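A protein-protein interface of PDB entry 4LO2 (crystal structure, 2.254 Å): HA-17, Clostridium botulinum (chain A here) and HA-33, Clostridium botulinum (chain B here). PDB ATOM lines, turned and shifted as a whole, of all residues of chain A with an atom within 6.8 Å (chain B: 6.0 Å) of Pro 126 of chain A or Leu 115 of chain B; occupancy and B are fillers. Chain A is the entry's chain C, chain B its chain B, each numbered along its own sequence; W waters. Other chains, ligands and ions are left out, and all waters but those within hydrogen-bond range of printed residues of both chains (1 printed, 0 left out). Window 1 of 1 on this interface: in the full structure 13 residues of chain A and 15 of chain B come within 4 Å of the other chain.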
ATOM      1  N   SER A  32     -10.422   4.094  19.818  1.00  0.00           N
ATOM      2  CA  SER A  32      -9.851   5.277  20.467  1.00  0.00           C
ATOM      3  C   SER A  32     -10.728   6.496  20.276  1.00  0.00           C
ATOM      4  O   SER A  32     -11.672   6.494  19.485  1.00  0.00           O
ATOM      5  CB  SER A  32      -8.459   5.603  19.910  1.00  0.00           C
ATOM      6  OG  SER A  32      -7.600   4.490  19.974  1.00  0.00           O
ATOM      7  N   LEU A  33     -10.383   7.548  21.005  1.00  0.00           N
ATOM      8  CA  LEU A  33     -11.010   8.853  20.865  1.00  0.00           C
ATOM      9  C   LEU A  33      -9.960   9.804  20.295  1.00  0.00           C
ATOM     10  O   LEU A  33      -8.805   9.787  20.730  1.00  0.00           O
ATOM     11  CB  LEU A  33     -11.474   9.371  22.238  1.00  0.00           C
ATOM     12  CG  LEU A  33     -12.813   8.870  22.790  1.00  0.00           C
ATOM     13  CD1 LEU A  33     -13.945   9.128  21.759  1.00  0.00           C
ATOM     14  CD2 LEU A  33     -12.767   7.390  23.187  1.00  0.00           C
ATOM     15  N   THR A  34     -10.349  10.641  19.342  1.00  0.00           N
ATOM     16  CA  THR A  34      -9.397  11.578  18.759  1.00  0.00           C
ATOM     17  C   THR A  34     -10.116  12.838  18.296  1.00  0.00           C
ATOM     18  O   THR A  34     -11.348  12.876  18.267  1.00  0.00           O
ATOM     19  CB  THR A  34      -8.623  10.938  17.577  1.00  0.00           C
ATOM     20  OG1 THR A  34      -7.411  11.668  17.332  1.00  0.00           O
ATOM     21  CG2 THR A  34      -9.477  10.906  16.295  1.00  0.00           C
ATOM     22  N   PHE A  35      -9.347  13.868  17.953  1.00  0.00           N
ATOM     23  CA  PHE A  35      -9.920  15.119  17.455  1.00  0.00           C
ATOM     24  C   PHE A  35      -9.763  15.205  15.941  1.00  0.00           C
ATOM     25  O   PHE A  35      -8.649  15.181  15.425  1.00  0.00           O
ATOM     26  CB  PHE A  35      -9.285  16.324  18.152  1.00  0.00           C
ATOM     27  CG  PHE A  35      -9.590  16.396  19.628  1.00  0.00           C
ATOM     28  CD1 PHE A  35     -10.716  17.067  20.079  1.00  0.00           C
ATOM     29  CD2 PHE A  35      -8.757  15.776  20.561  1.00  0.00           C
ATOM     30  CE1 PHE A  35     -11.014  17.126  21.427  1.00  0.00           C
ATOM     31  CE2 PHE A  35      -9.045  15.834  21.913  1.00  0.00           C
ATOM     32  CZ  PHE A  35     -10.172  16.508  22.346  1.00  0.00           C
ATOM     33  N   PHE A  74      -5.091   0.623  29.861  1.00  0.00           N
ATOM     34  CA  PHE A  74      -3.871   0.917  29.106  1.00  0.00           C
ATOM     35  C   PHE A  74      -3.584   2.418  29.002  1.00  0.00           C
ATOM     36  O   PHE A  74      -2.636   2.836  28.337  1.00  0.00           O
ATOM     37  CB  PHE A  74      -3.954   0.259  27.728  1.00  0.00           C
ATOM     38  CG  PHE A  74      -4.199  -1.218  27.807  1.00  0.00           C
ATOM     39  CD1 PHE A  74      -3.148  -2.094  28.035  1.00  0.00           C
ATOM     40  CD2 PHE A  74      -5.490  -1.725  27.720  1.00  0.00           C
ATOM     41  CE1 PHE A  74      -3.366  -3.452  28.143  1.00  0.00           C
ATOM     42  CE2 PHE A  74      -5.724  -3.090  27.828  1.00  0.00           C
ATOM     43  CZ  PHE A  74      -4.665  -3.955  28.041  1.00  0.00           C
ATOM     44  N   GLY A  75      -4.411   3.220  29.669  1.00  0.00           N
ATOM     45  CA  GLY A  75      -4.206   4.656  29.734  1.00  0.00           C
ATOM     46  C   GLY A  75      -5.039   5.434  28.728  1.00  0.00           C
ATOM     47  O   GLY A  75      -4.988   6.672  28.695  1.00  0.00           O
ATOM     48  N   PHE A  76      -5.814   4.720  27.908  1.00  0.00           N
ATOM     49  CA  PHE A  76      -6.636   5.362  26.881  1.00  0.00           C
ATOM     50  C   PHE A  76      -8.026   5.693  27.382  1.00  0.00           C
ATOM     51  O   PHE A  76      -8.639   4.893  28.094  1.00  0.00           O
ATOM     52  CB  PHE A  76      -6.825   4.428  25.687  1.00  0.00           C
ATOM     53  CG  PHE A  76      -5.623   4.286  24.825  1.00  0.00           C
ATOM     54  CD1 PHE A  76      -4.562   3.497  25.226  1.00  0.00           C
ATOM     55  CD2 PHE A  76      -5.567   4.911  23.587  1.00  0.00           C
ATOM     56  CE1 PHE A  76      -3.451   3.352  24.420  1.00  0.00           C
ATOM     57  CE2 PHE A  76      -4.452   4.773  22.773  1.00  0.00           C
ATOM     58  CZ  PHE A  76      -3.392   3.988  23.192  1.00  0.00           C
ATOM     59  N   ILE A  77      -8.535   6.856  26.982  1.00  0.00           N
ATOM     60  CA  ILE A  77      -9.966   7.125  27.077  1.00  0.00           C
ATOM     61  C   ILE A  77     -10.687   6.222  26.060  1.00  0.00           C
ATOM     62  O   ILE A  77     -10.213   6.026  24.928  1.00  0.00           O
ATOM     63  CB  ILE A  77     -10.286   8.614  26.790  1.00  0.00           C
ATOM     64  CG1 ILE A  77      -9.511   9.519  27.758  1.00  0.00           C
ATOM     65  CG2 ILE A  77     -11.808   8.894  26.904  1.00  0.00           C
ATOM     66  CD1 ILE A  77      -9.777   9.188  29.217  1.00  0.00           C
ATOM     67  N   ASP A 114      -6.162  13.899  28.697  1.00  0.00           N
ATOM     68  CA  ASP A 114      -4.892  14.511  28.323  1.00  0.00           C
ATOM     69  C   ASP A 114      -4.647  14.246  26.845  1.00  0.00           C
ATOM     70  O   ASP A 114      -4.723  13.114  26.386  1.00  0.00           O
ATOM     71  CB  ASP A 114      -3.759  13.936  29.187  1.00  0.00           C
ATOM     72  CG  ASP A 114      -2.448  14.711  29.051  1.00  0.00           C
ATOM     73  OD1 ASP A 114      -1.895  14.776  27.925  1.00  0.00           O
ATOM     74  OD2 ASP A 114      -1.953  15.230  30.082  1.00  0.00           O
ATOM     75  N   ILE A 115      -4.376  15.302  26.095  1.00  0.00           N
ATOM     76  CA  ILE A 115      -4.092  15.162  24.677  1.00  0.00           C
ATOM     77  C   ILE A 115      -2.661  15.658  24.430  1.00  0.00           C
ATOM     78  O   ILE A 115      -2.293  16.758  24.851  1.00  0.00           O
ATOM     79  CB  ILE A 115      -5.144  15.907  23.786  1.00  0.00           C
ATOM     80  CG1 ILE A 115      -5.019  15.498  22.309  1.00  0.00           C
ATOM     81  CG2 ILE A 115      -5.055  17.422  23.957  1.00  0.00           C
ATOM     82  CD1 ILE A 115      -5.435  14.063  22.035  1.00  0.00           C
ATOM     83  N   TYR A 116      -1.846  14.825  23.783  1.00  0.00           N
ATOM     84  CA  TYR A 116      -0.449  15.170  23.522  1.00  0.00           C
ATOM     85  C   TYR A 116      -0.346  16.039  22.283  1.00  0.00           C
ATOM     86  O   TYR A 116      -1.027  15.793  21.293  1.00  0.00           O
ATOM     87  CB  TYR A 116       0.390  13.908  23.328  1.00  0.00           C
ATOM     88  CG  TYR A 116       1.880  14.165  23.282  1.00  0.00           C
ATOM     89  CD1 TYR A 116       2.528  14.388  22.077  1.00  0.00           C
ATOM     90  CD2 TYR A 116       2.638  14.191  24.453  1.00  0.00           C
ATOM     91  CE1 TYR A 116       3.892  14.623  22.029  1.00  0.00           C
ATOM     92  CE2 TYR A 116       4.001  14.428  24.414  1.00  0.00           C
ATOM     93  CZ  TYR A 116       4.620  14.636  23.203  1.00  0.00           C
ATOM     94  OH  TYR A 116       5.967  14.869  23.156  1.00  0.00           O
ATOM     95  N   ILE A 122      -2.312  18.309  17.319  1.00  0.00           N
ATOM     96  CA  ILE A 122      -2.857  17.111  17.970  1.00  0.00           C
ATOM     97  C   ILE A 122      -3.471  16.085  16.997  1.00  0.00           C
ATOM     98  O   ILE A 122      -4.110  15.114  17.423  1.00  0.00           O
ATOM     99  CB  ILE A 122      -3.926  17.481  19.026  1.00  0.00           C
ATOM    100  CG1 ILE A 122      -5.111  18.198  18.361  1.00  0.00           C
ATOM    101  CG2 ILE A 122      -3.303  18.341  20.127  1.00  0.00           C
ATOM    102  CD1 ILE A 122      -6.300  18.419  19.285  1.00  0.00           C
ATOM    103  N   LEU A 123      -3.270  16.298  15.700  1.00  0.00           N
ATOM    104  CA  LEU A 123      -3.810  15.400  14.680  1.00  0.00           C
ATOM    105  C   LEU A 123      -3.357  13.962  14.904  1.00  0.00           C
ATOM    106  O   LEU A 123      -2.167  13.693  15.084  1.00  0.00           O
ATOM    107  CB  LEU A 123      -3.390  15.857  13.281  1.00  0.00           C
ATOM    108  CG  LEU A 123      -4.471  16.178  12.240  1.00  0.00           C
ATOM    109  CD1 LEU A 123      -4.013  15.694  10.863  1.00  0.00           C
ATOM    110  CD2 LEU A 123      -5.840  15.592  12.589  1.00  0.00           C
ATOM    111  N   SER A 124      -4.327  13.052  14.907  1.00  0.00           N
ATOM    112  CA  SER A 124      -4.083  11.614  15.030  1.00  0.00           C
ATOM    113  C   SER A 124      -3.684  11.164  16.423  1.00  0.00           C
ATOM    114  O   SER A 124      -3.407   9.981  16.624  1.00  0.00           O
ATOM    115  CB  SER A 124      -3.054  11.120  14.000  1.00  0.00           C
ATOM    116  OG  SER A 124      -3.406  11.556  12.705  1.00  0.00           O
ATOM    117  N   GLN A 125      -3.657  12.091  17.383  1.00  0.00           N
ATOM    118  CA  GLN A 125      -3.378  11.724  18.767  1.00  0.00           C
ATOM    119  C   GLN A 125      -4.619  11.140  19.431  1.00  0.00           C
ATOM    120  O   GLN A 125      -5.709  11.694  19.309  1.00  0.00           O
ATOM    121  CB  GLN A 125      -2.883  12.936  19.588  1.00  0.00           C
ATOM    122  CG  GLN A 125      -1.488  13.468  19.179  1.00  0.00           C
ATOM    123  CD  GLN A 125      -0.353  12.526  19.540  1.00  0.00           C
ATOM    124  OE1 GLN A 125      -0.546  11.541  20.254  1.00  0.00           O
ATOM    125  NE2 GLN A 125       0.847  12.829  19.046  1.00  0.00           N
ATOM    126  N   PRO A 126      -4.451  10.025  20.160  1.00  0.00           N
ATOM    127  CA  PRO A 126      -5.561   9.506  20.953  1.00  0.00           C
ATOM    128  C   PRO A 126      -5.651  10.238  22.306  1.00  0.00           C
ATOM    129  O   PRO A 126      -4.646  10.668  22.891  1.00  0.00           O
ATOM    130  CB  PRO A 126      -5.148   8.054  21.191  1.00  0.00           C
ATOM    131  CG  PRO A 126      -3.606   8.162  21.369  1.00  0.00           C
ATOM    132  CD  PRO A 126      -3.211   9.241  20.354  1.00  0.00           C
ATOM    133  N   LEU A 127      -6.864  10.368  22.809  1.00  0.00           N
ATOM    134  CA  LEU A 127      -7.070  10.964  24.114  1.00  0.00           C
ATOM    135  C   LEU A 127      -6.679   9.963  25.196  1.00  0.00           C
ATOM    136  O   LEU A 127      -7.148   8.818  25.196  1.00  0.00           O
ATOM    137  CB  LEU A 127      -8.533  11.405  24.251  1.00  0.00           C
ATOM    138  CG  LEU A 127      -8.978  12.254  25.446  1.00  0.00           C
ATOM    139  CD1 LEU A 127      -8.222  13.569  25.482  1.00  0.00           C
ATOM    140  CD2 LEU A 127     -10.503  12.496  25.326  1.00  0.00           C
ATOM    141  N   LEU A 128      -5.811  10.401  26.111  1.00  0.00           N
ATOM    142  CA  LEU A 128      -5.327   9.559  27.203  1.00  0.00           C
ATOM    143  C   LEU A 128      -5.838  10.009  28.574  1.00  0.00           C
ATOM    144  O   LEU A 128      -6.449  11.085  28.724  1.00  0.00           O
ATOM    145  CB  LEU A 128      -3.798   9.531  27.215  1.00  0.00           C
ATOM    146  CG  LEU A 128      -3.123   9.167  25.884  1.00  0.00           C
ATOM    147  CD1 LEU A 128      -1.595   9.102  26.047  1.00  0.00           C
ATOM    148  CD2 LEU A 128      -3.671   7.859  25.329  1.00  0.00           C
ATOM    149  N   TRP B  74       2.997   2.792  14.176  1.00  0.00           N
ATOM    150  CA  TRP B  74       1.810   2.943  15.020  1.00  0.00           C
ATOM    151  C   TRP B  74       0.712   3.586  14.189  1.00  0.00           C
ATOM    152  O   TRP B  74       0.872   4.701  13.675  1.00  0.00           O
ATOM    153  CB  TRP B  74       2.104   3.810  16.240  1.00  0.00           C
ATOM    154  CG  TRP B  74       0.850   4.252  17.017  1.00  0.00           C
ATOM    155  CD1 TRP B  74      -0.327   3.567  17.152  1.00  0.00           C
ATOM    156  CD2 TRP B  74       0.680   5.483  17.743  1.00  0.00           C
ATOM    157  NE1 TRP B  74      -1.212   4.288  17.914  1.00  0.00           N
ATOM    158  CE2 TRP B  74      -0.619   5.463  18.299  1.00  0.00           C
ATOM    159  CE3 TRP B  74       1.506   6.587  17.990  1.00  0.00           C
ATOM    160  CZ2 TRP B  74      -1.119   6.511  19.072  1.00  0.00           C
ATOM    161  CZ3 TRP B  74       1.010   7.630  18.763  1.00  0.00           C
ATOM    162  CH2 TRP B  74      -0.297   7.588  19.288  1.00  0.00           C
ATOM    163  N   ALA B  76      -1.732   5.457  14.577  1.00  0.00           N
ATOM    164  CA  ALA B  76      -2.388   6.473  15.397  1.00  0.00           C
ATOM    165  C   ALA B  76      -3.653   7.002  14.713  1.00  0.00           C
ATOM    166  O   ALA B  76      -3.643   7.245  13.520  1.00  0.00           O
ATOM    167  CB  ALA B  76      -1.407   7.617  15.697  1.00  0.00           C
ATOM    168  N   PRO B  77      -4.739   7.204  15.478  1.00  0.00           N
ATOM    169  CA  PRO B  77      -4.805   7.132  16.944  1.00  0.00           C
ATOM    170  C   PRO B  77      -5.224   5.767  17.486  1.00  0.00           C
ATOM    171  O   PRO B  77      -5.498   5.654  18.684  1.00  0.00           O
ATOM    172  CB  PRO B  77      -5.898   8.143  17.272  1.00  0.00           C
ATOM    173  CG  PRO B  77      -6.874   7.975  16.101  1.00  0.00           C
ATOM    174  CD  PRO B  77      -6.025   7.641  14.893  1.00  0.00           C
ATOM    175  N   THR B  78      -5.279   4.750  16.640  1.00  0.00           N
ATOM    176  CA  THR B  78      -5.783   3.453  17.085  1.00  0.00           C
ATOM    177  C   THR B  78      -4.775   2.742  17.975  1.00  0.00           C
ATOM    178  O   THR B  78      -3.645   3.200  18.141  1.00  0.00           O
ATOM    179  CB  THR B  78      -6.095   2.533  15.893  1.00  0.00           C
ATOM    180  OG1 THR B  78      -4.864   2.031  15.352  1.00  0.00           O
ATOM    181  CG2 THR B  78      -6.849   3.303  14.822  1.00  0.00           C
ATOM    182  N   TRP B  94      10.757   5.388  17.109  1.00  0.00           N
ATOM    183  CA  TRP B  94      10.636   4.718  18.396  1.00  0.00           C
ATOM    184  C   TRP B  94      11.839   5.031  19.276  1.00  0.00           C
ATOM    185  O   TRP B  94      12.979   5.044  18.805  1.00  0.00           O
ATOM    186  CB  TRP B  94      10.528   3.203  18.187  1.00  0.00           C
ATOM    187  CG  TRP B  94       9.398   2.852  17.306  1.00  0.00           C
ATOM    188  CD1 TRP B  94       9.430   2.687  15.947  1.00  0.00           C
ATOM    189  CD2 TRP B  94       8.041   2.638  17.709  1.00  0.00           C
ATOM    190  NE1 TRP B  94       8.177   2.386  15.490  1.00  0.00           N
ATOM    191  CE2 TRP B  94       7.306   2.348  16.547  1.00  0.00           C
ATOM    192  CE3 TRP B  94       7.380   2.664  18.942  1.00  0.00           C
ATOM    193  CZ2 TRP B  94       5.930   2.081  16.573  1.00  0.00           C
ATOM    194  CZ3 TRP B  94       6.008   2.407  18.968  1.00  0.00           C
ATOM    195  CH2 TRP B  94       5.301   2.119  17.788  1.00  0.00           C
ATOM    196  N   ILE B 107       9.944   0.159  24.523  1.00  0.00           N
ATOM    197  CA  ILE B 107       9.928   0.735  23.183  1.00  0.00           C
ATOM    198  C   ILE B 107       8.798   1.759  23.067  1.00  0.00           C
ATOM    199  O   ILE B 107       7.634   1.387  22.935  1.00  0.00           O
ATOM    200  CB  ILE B 107       9.779  -0.367  22.129  1.00  0.00           C
ATOM    201  CG1 ILE B 107      10.922  -1.385  22.274  1.00  0.00           C
ATOM    202  CG2 ILE B 107       9.747   0.229  20.728  1.00  0.00           C
ATOM    203  CD1 ILE B 107      10.732  -2.644  21.406  1.00  0.00           C
ATOM    204  N   ALA B 108       9.154   3.044  23.128  1.00  0.00           N
ATOM    205  CA  ALA B 108       8.173   4.122  23.254  1.00  0.00           C
ATOM    206  C   ALA B 108       7.941   4.835  21.928  1.00  0.00           C
ATOM    207  O   ALA B 108       8.873   5.041  21.168  1.00  0.00           O
ATOM    208  CB  ALA B 108       8.629   5.149  24.350  1.00  0.00           C
ATOM    209  N   SER B 109       6.710   5.245  21.647  1.00  0.00           N
ATOM    210  CA  SER B 109       6.469   5.931  20.374  1.00  0.00           C
ATOM    211  C   SER B 109       7.068   7.328  20.386  1.00  0.00           C
ATOM    212  O   SER B 109       6.889   8.075  21.342  1.00  0.00           O
ATOM    213  CB  SER B 109       4.976   6.051  20.083  1.00  0.00           C
ATOM    214  OG  SER B 109       4.753   6.970  19.016  1.00  0.00           O
ATOM    215  N   ASN B 112       4.150   9.880  20.380  1.00  0.00           N
ATOM    216  CA  ASN B 112       3.594  10.113  21.711  1.00  0.00           C
ATOM    217  C   ASN B 112       4.334   9.247  22.726  1.00  0.00           C
ATOM    218  O   ASN B 112       3.969   8.098  22.954  1.00  0.00           O
ATOM    219  CB  ASN B 112       2.096   9.806  21.736  1.00  0.00           C
ATOM    220  CG  ASN B 112       1.416  10.294  23.018  1.00  0.00           C
ATOM    221  OD1 ASN B 112       2.043  10.385  24.083  1.00  0.00           O
ATOM    222  ND2 ASN B 112       0.122  10.599  22.920  1.00  0.00           N
ATOM    223  N   PRO B 113       5.387   9.804  23.337  1.00  0.00           N
ATOM    224  CA  PRO B 113       6.280   9.080  24.247  1.00  0.00           C
ATOM    225  C   PRO B 113       5.605   8.603  25.528  1.00  0.00           C
ATOM    226  O   PRO B 113       6.210   7.809  26.236  1.00  0.00           O
ATOM    227  CB  PRO B 113       7.367  10.107  24.582  1.00  0.00           C
ATOM    228  CG  PRO B 113       7.253  11.155  23.568  1.00  0.00           C
ATOM    229  CD  PRO B 113       5.831  11.181  23.100  1.00  0.00           C
ATOM    230  N   ASN B 114       4.395   9.075  25.832  1.00  0.00           N
ATOM    231  CA  ASN B 114       3.607   8.464  26.904  1.00  0.00           C
ATOM    232  C   ASN B 114       3.138   7.041  26.592  1.00  0.00           C
ATOM    233  O   ASN B 114       2.650   6.327  27.483  1.00  0.00           O
ATOM    234  CB  ASN B 114       2.387   9.326  27.242  1.00  0.00           C
ATOM    235  CG  ASN B 114       2.774  10.714  27.714  1.00  0.00           C
ATOM    236  OD1 ASN B 114       2.575  11.700  27.006  1.00  0.00           O
ATOM    237  ND2 ASN B 114       3.320  10.801  28.913  1.00  0.00           N
ATOM    238  N   LEU B 115       3.263   6.637  25.333  1.00  0.00           N
ATOM    239  CA  LEU B 115       2.771   5.337  24.898  1.00  0.00           C
ATOM    240  C   LEU B 115       3.909   4.440  24.466  1.00  0.00           C
ATOM    241  O   LEU B 115       4.788   4.859  23.728  1.00  0.00           O
ATOM    242  CB  LEU B 115       1.776   5.497  23.739  1.00  0.00           C
ATOM    243  CG  LEU B 115       0.503   6.240  24.113  1.00  0.00           C
ATOM    244  CD1 LEU B 115      -0.366   6.403  22.866  1.00  0.00           C
ATOM    245  CD2 LEU B 115      -0.239   5.479  25.228  1.00  0.00           C
ATOM    246  N   VAL B 116       3.876   3.194  24.929  1.00  0.00           N
ATOM    247  CA  VAL B 116       4.932   2.235  24.661  1.00  0.00           C
ATOM    248  C   VAL B 116       4.304   0.914  24.174  1.00  0.00           C
ATOM    249  O   VAL B 116       3.133   0.621  24.459  1.00  0.00           O
ATOM    250  CB  VAL B 116       5.812   1.999  25.939  1.00  0.00           C
ATOM    251  CG1 VAL B 116       6.288   3.337  26.523  1.00  0.00           C
ATOM    252  CG2 VAL B 116       5.020   1.238  27.009  1.00  0.00           C
ATOM    253  N   LEU B 117       5.084   0.130  23.431  1.00  0.00           N
ATOM    254  CA  LEU B 117       4.633  -1.168  22.936  1.00  0.00           C
ATOM    255  C   LEU B 117       4.318  -2.096  24.092  1.00  0.00           C
ATOM    256  O   LEU B 117       5.026  -2.123  25.110  1.00  0.00           O
ATOM    257  CB  LEU B 117       5.677  -1.813  22.015  1.00  0.00           C
ATOM    258  CG  LEU B 117       6.014  -1.125  20.688  1.00  0.00           C
ATOM    259  CD1 LEU B 117       7.043  -1.942  19.889  1.00  0.00           C
ATOM    260  CD2 LEU B 117       4.757  -0.920  19.859  1.00  0.00           C
ATOM    261  N   LEU B 128      -0.542  -0.797  22.559  1.00  0.00           N
ATOM    262  CA  LEU B 128       0.131   0.317  23.202  1.00  0.00           C
ATOM    263  C   LEU B 128      -0.372   0.491  24.624  1.00  0.00           C
ATOM    264  O   LEU B 128      -1.467   0.105  24.948  1.00  0.00           O
ATOM    265  CB  LEU B 128      -0.089   1.615  22.426  1.00  0.00           C
ATOM    266  CG  LEU B 128       0.622   1.834  21.086  1.00  0.00           C
ATOM    267  CD1 LEU B 128       0.229   3.188  20.573  1.00  0.00           C
ATOM    268  CD2 LEU B 128       2.133   1.771  21.208  1.00  0.00           C
ATOM    269  N   SER B 129       0.450   1.075  25.483  1.00  0.00           N
ATOM    270  CA  SER B 129       0.047   1.293  26.852  1.00  0.00           C
ATOM    271  C   SER B 129       0.848   2.456  27.384  1.00  0.00           C
ATOM    272  O   SER B 129       1.933   2.745  26.896  1.00  0.00           O
ATOM    273  CB  SER B 129       0.334   0.043  27.695  1.00  0.00           C
ATOM    274  OG  SER B 129       0.140   0.285  29.078  1.00  0.00           O
ATOM    275  N   THR B 130       0.312   3.130  28.385  1.00  0.00           N
ATOM    276  CA  THR B 130       1.132   4.047  29.130  1.00  0.00           C
ATOM    277  C   THR B 130       2.083   3.211  29.990  1.00  0.00           C
ATOM    278  O   THR B 130       1.891   2.003  30.161  1.00  0.00           O
ATOM    279  CB  THR B 130       0.264   4.964  29.982  1.00  0.00           C
ATOM    280  OG1 THR B 130      -0.649   4.167  30.753  1.00  0.00           O
ATOM    281  CG2 THR B 130      -0.529   5.910  29.066  1.00  0.00           C
ATOM    282  N   LEU B 131       3.124   3.850  30.499  1.00  0.00           N
ATOM    283  CA  LEU B 131       4.194   3.164  31.202  1.00  0.00           C
ATOM    284  C   LEU B 131       3.709   2.568  32.523  1.00  0.00           C
ATOM    285  O   LEU B 131       2.946   3.184  33.229  1.00  0.00           O
ATOM    286  CB  LEU B 131       5.307   4.158  31.493  1.00  0.00           C
ATOM    287  CG  LEU B 131       6.517   4.255  30.586  1.00  0.00           C
ATOM    288  CD1 LEU B 131       7.396   5.399  31.100  1.00  0.00           C
ATOM    289  CD2 LEU B 131       7.280   2.963  30.664  1.00  0.00           C
HETATM  290  O   HOH W   1      -2.405  12.009  23.615  1.00  0.00           O
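The backbone nitrogen (N) of Pro 77 of chain B lies close to the backbone carbonyl oxygen (O) of Ser 124 of chain A. The backbone NH (N) of Thr 130 of chain B lies within hydrogen-bond range of the backbone carbonyl oxygen (O) of Phe 74 of chain A (3.0 Å). OG of Ser 32 of chain A lies within hydrogen-bond range of O of Pro 77 of chain B, at 2.7 Å. The side-chain amide oxygen (OE1) of Gln 125 of chain A sits at hydrogen-bond distance from the side-chain amide nitrogen (ND2) of Asn 112 of chain B (2.9 Å).
O of Gln 125 of chain A is in hydrogen-bond range of OG1 of Thr 34 of chain A, 2.6 Å away. NE1 of Trp 74 of chain B is in hydrogen-bond range of O of Thr 78 of chain B (2.7 Å). O of Ser 129 of chain B sits at hydrogen-bond distance from N of Val 116 of chain B, 2.8 Å away. The side-chain hydroxyl (OG) of Ser 109 of chain B sits at hydrogen-bond distance from the backbone NH (N) of Asn 112 of chain B, 3.3 Å away. The backbone NH of Ser 109 of chain B is in hydrogen-bond range of the backbone carbonyl oxygen of Leu 115 of chain B (2.9 Å). N of Asp 114 of chain A lies within hydrogen-bond range of O of Leu 128 of chain A.
Thr 34 of chain A touches Pro 77 of chain B. Phe 74 of chain A touches Leu 128 of chain B. Ser 129 of chain B touches Phe 74 of chain A (CA to O, 3.4 Å). Pro 113 of chain B touches Tyr 116 of chain A (CD to CZ, 3.7 Å). CD2 of Tyr 116 of chain A touches OD1 of Asn 114 of chain B (3.6 Å). CB of Ala 76 of chain B touches O of Ser 124 of chain A, at 3.2 Å. CB of Pro 77 of chain B touches C of Gln 125 of chain A, 3.9 Å away. CD of Pro 126 of chain A touches CH2 of Trp 74 of chain B, 3.5 Å away. Leu 115 of chain B touches Pro 126 of chain A (CD1 to CG, 3.98 Å). Asn 112 of chain B touches Leu 128 of chain A.
Of the printed residues of chain B, Phe 74 of chain A touches Leu 128 (3.7 Å), Ser 129 (3.4 Å) and Thr 130 (3.0 Å). Of chain B, only Trp 74, Pro 77 and Leu 115 come within 4 Å of Pro 126 of chain A. Printed residues of chain A within 4 Å of Trp 74 of chain B: Pro 126 (3.5 Å). Of the printed residues of chain A, Leu 115 of chain B touches Phe 76, Pro 126 and Leu 128. Leu 117 of chain B touches none of the printed residues of chain A. Of the printed residues of chain A, Leu 128 of chain B touches Phe 74 (3.7 Å) and Phe 76 (3.8 Å). Leu 131 of chain B touches none of the printed residues of chain A. The nearest residue of chain B that does not touch Pro 126 of chain A is Asn 112 of chain B (4.4 Å). The nearest residue of chain A that does not touch Leu 115 of chain B is Phe 74 of chain A (4.7 Å). The nearest printed residue of chain B that does not touch Phe 74 of chain A is Leu 115 of chain B (4.7 Å).
Of the 18 printed residues of chain B, 11 touch a printed residue of chain A. Hydrophobic or aromatic side chains of chain B within 4 Å of the printed part of chain A: Trp 74, Ala 76, Pro 77, Pro 113 and Leu 115. Of the 18 printed residues of chain A, 10 touch a printed residue of chain B. Printed residues of chain A that touch a printed residue of chain B: Ser 32, Thr 34, Phe 74, Gly 75, Phe 76, Tyr 116, Ser 124, Gln 125, Pro 126 and Leu 128. Hydrophobic or aromatic side chains of chain A that line the printed part of chain B: Phe 74, Phe 76, Tyr 116, Pro 126 and Leu 128. Among the printed residues, 21 pairs touch across the chains. Among the printed residues, no Asp or Glu carboxylate lies within 4 Å of a Lys or Arg side-chain nitrogen of the other chain.
Water W1 lies within hydrogen-bond range of O of Pro 126 of chain A, N of Tyr 116 of chain A and ND2 of Asn 112 of chain B.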
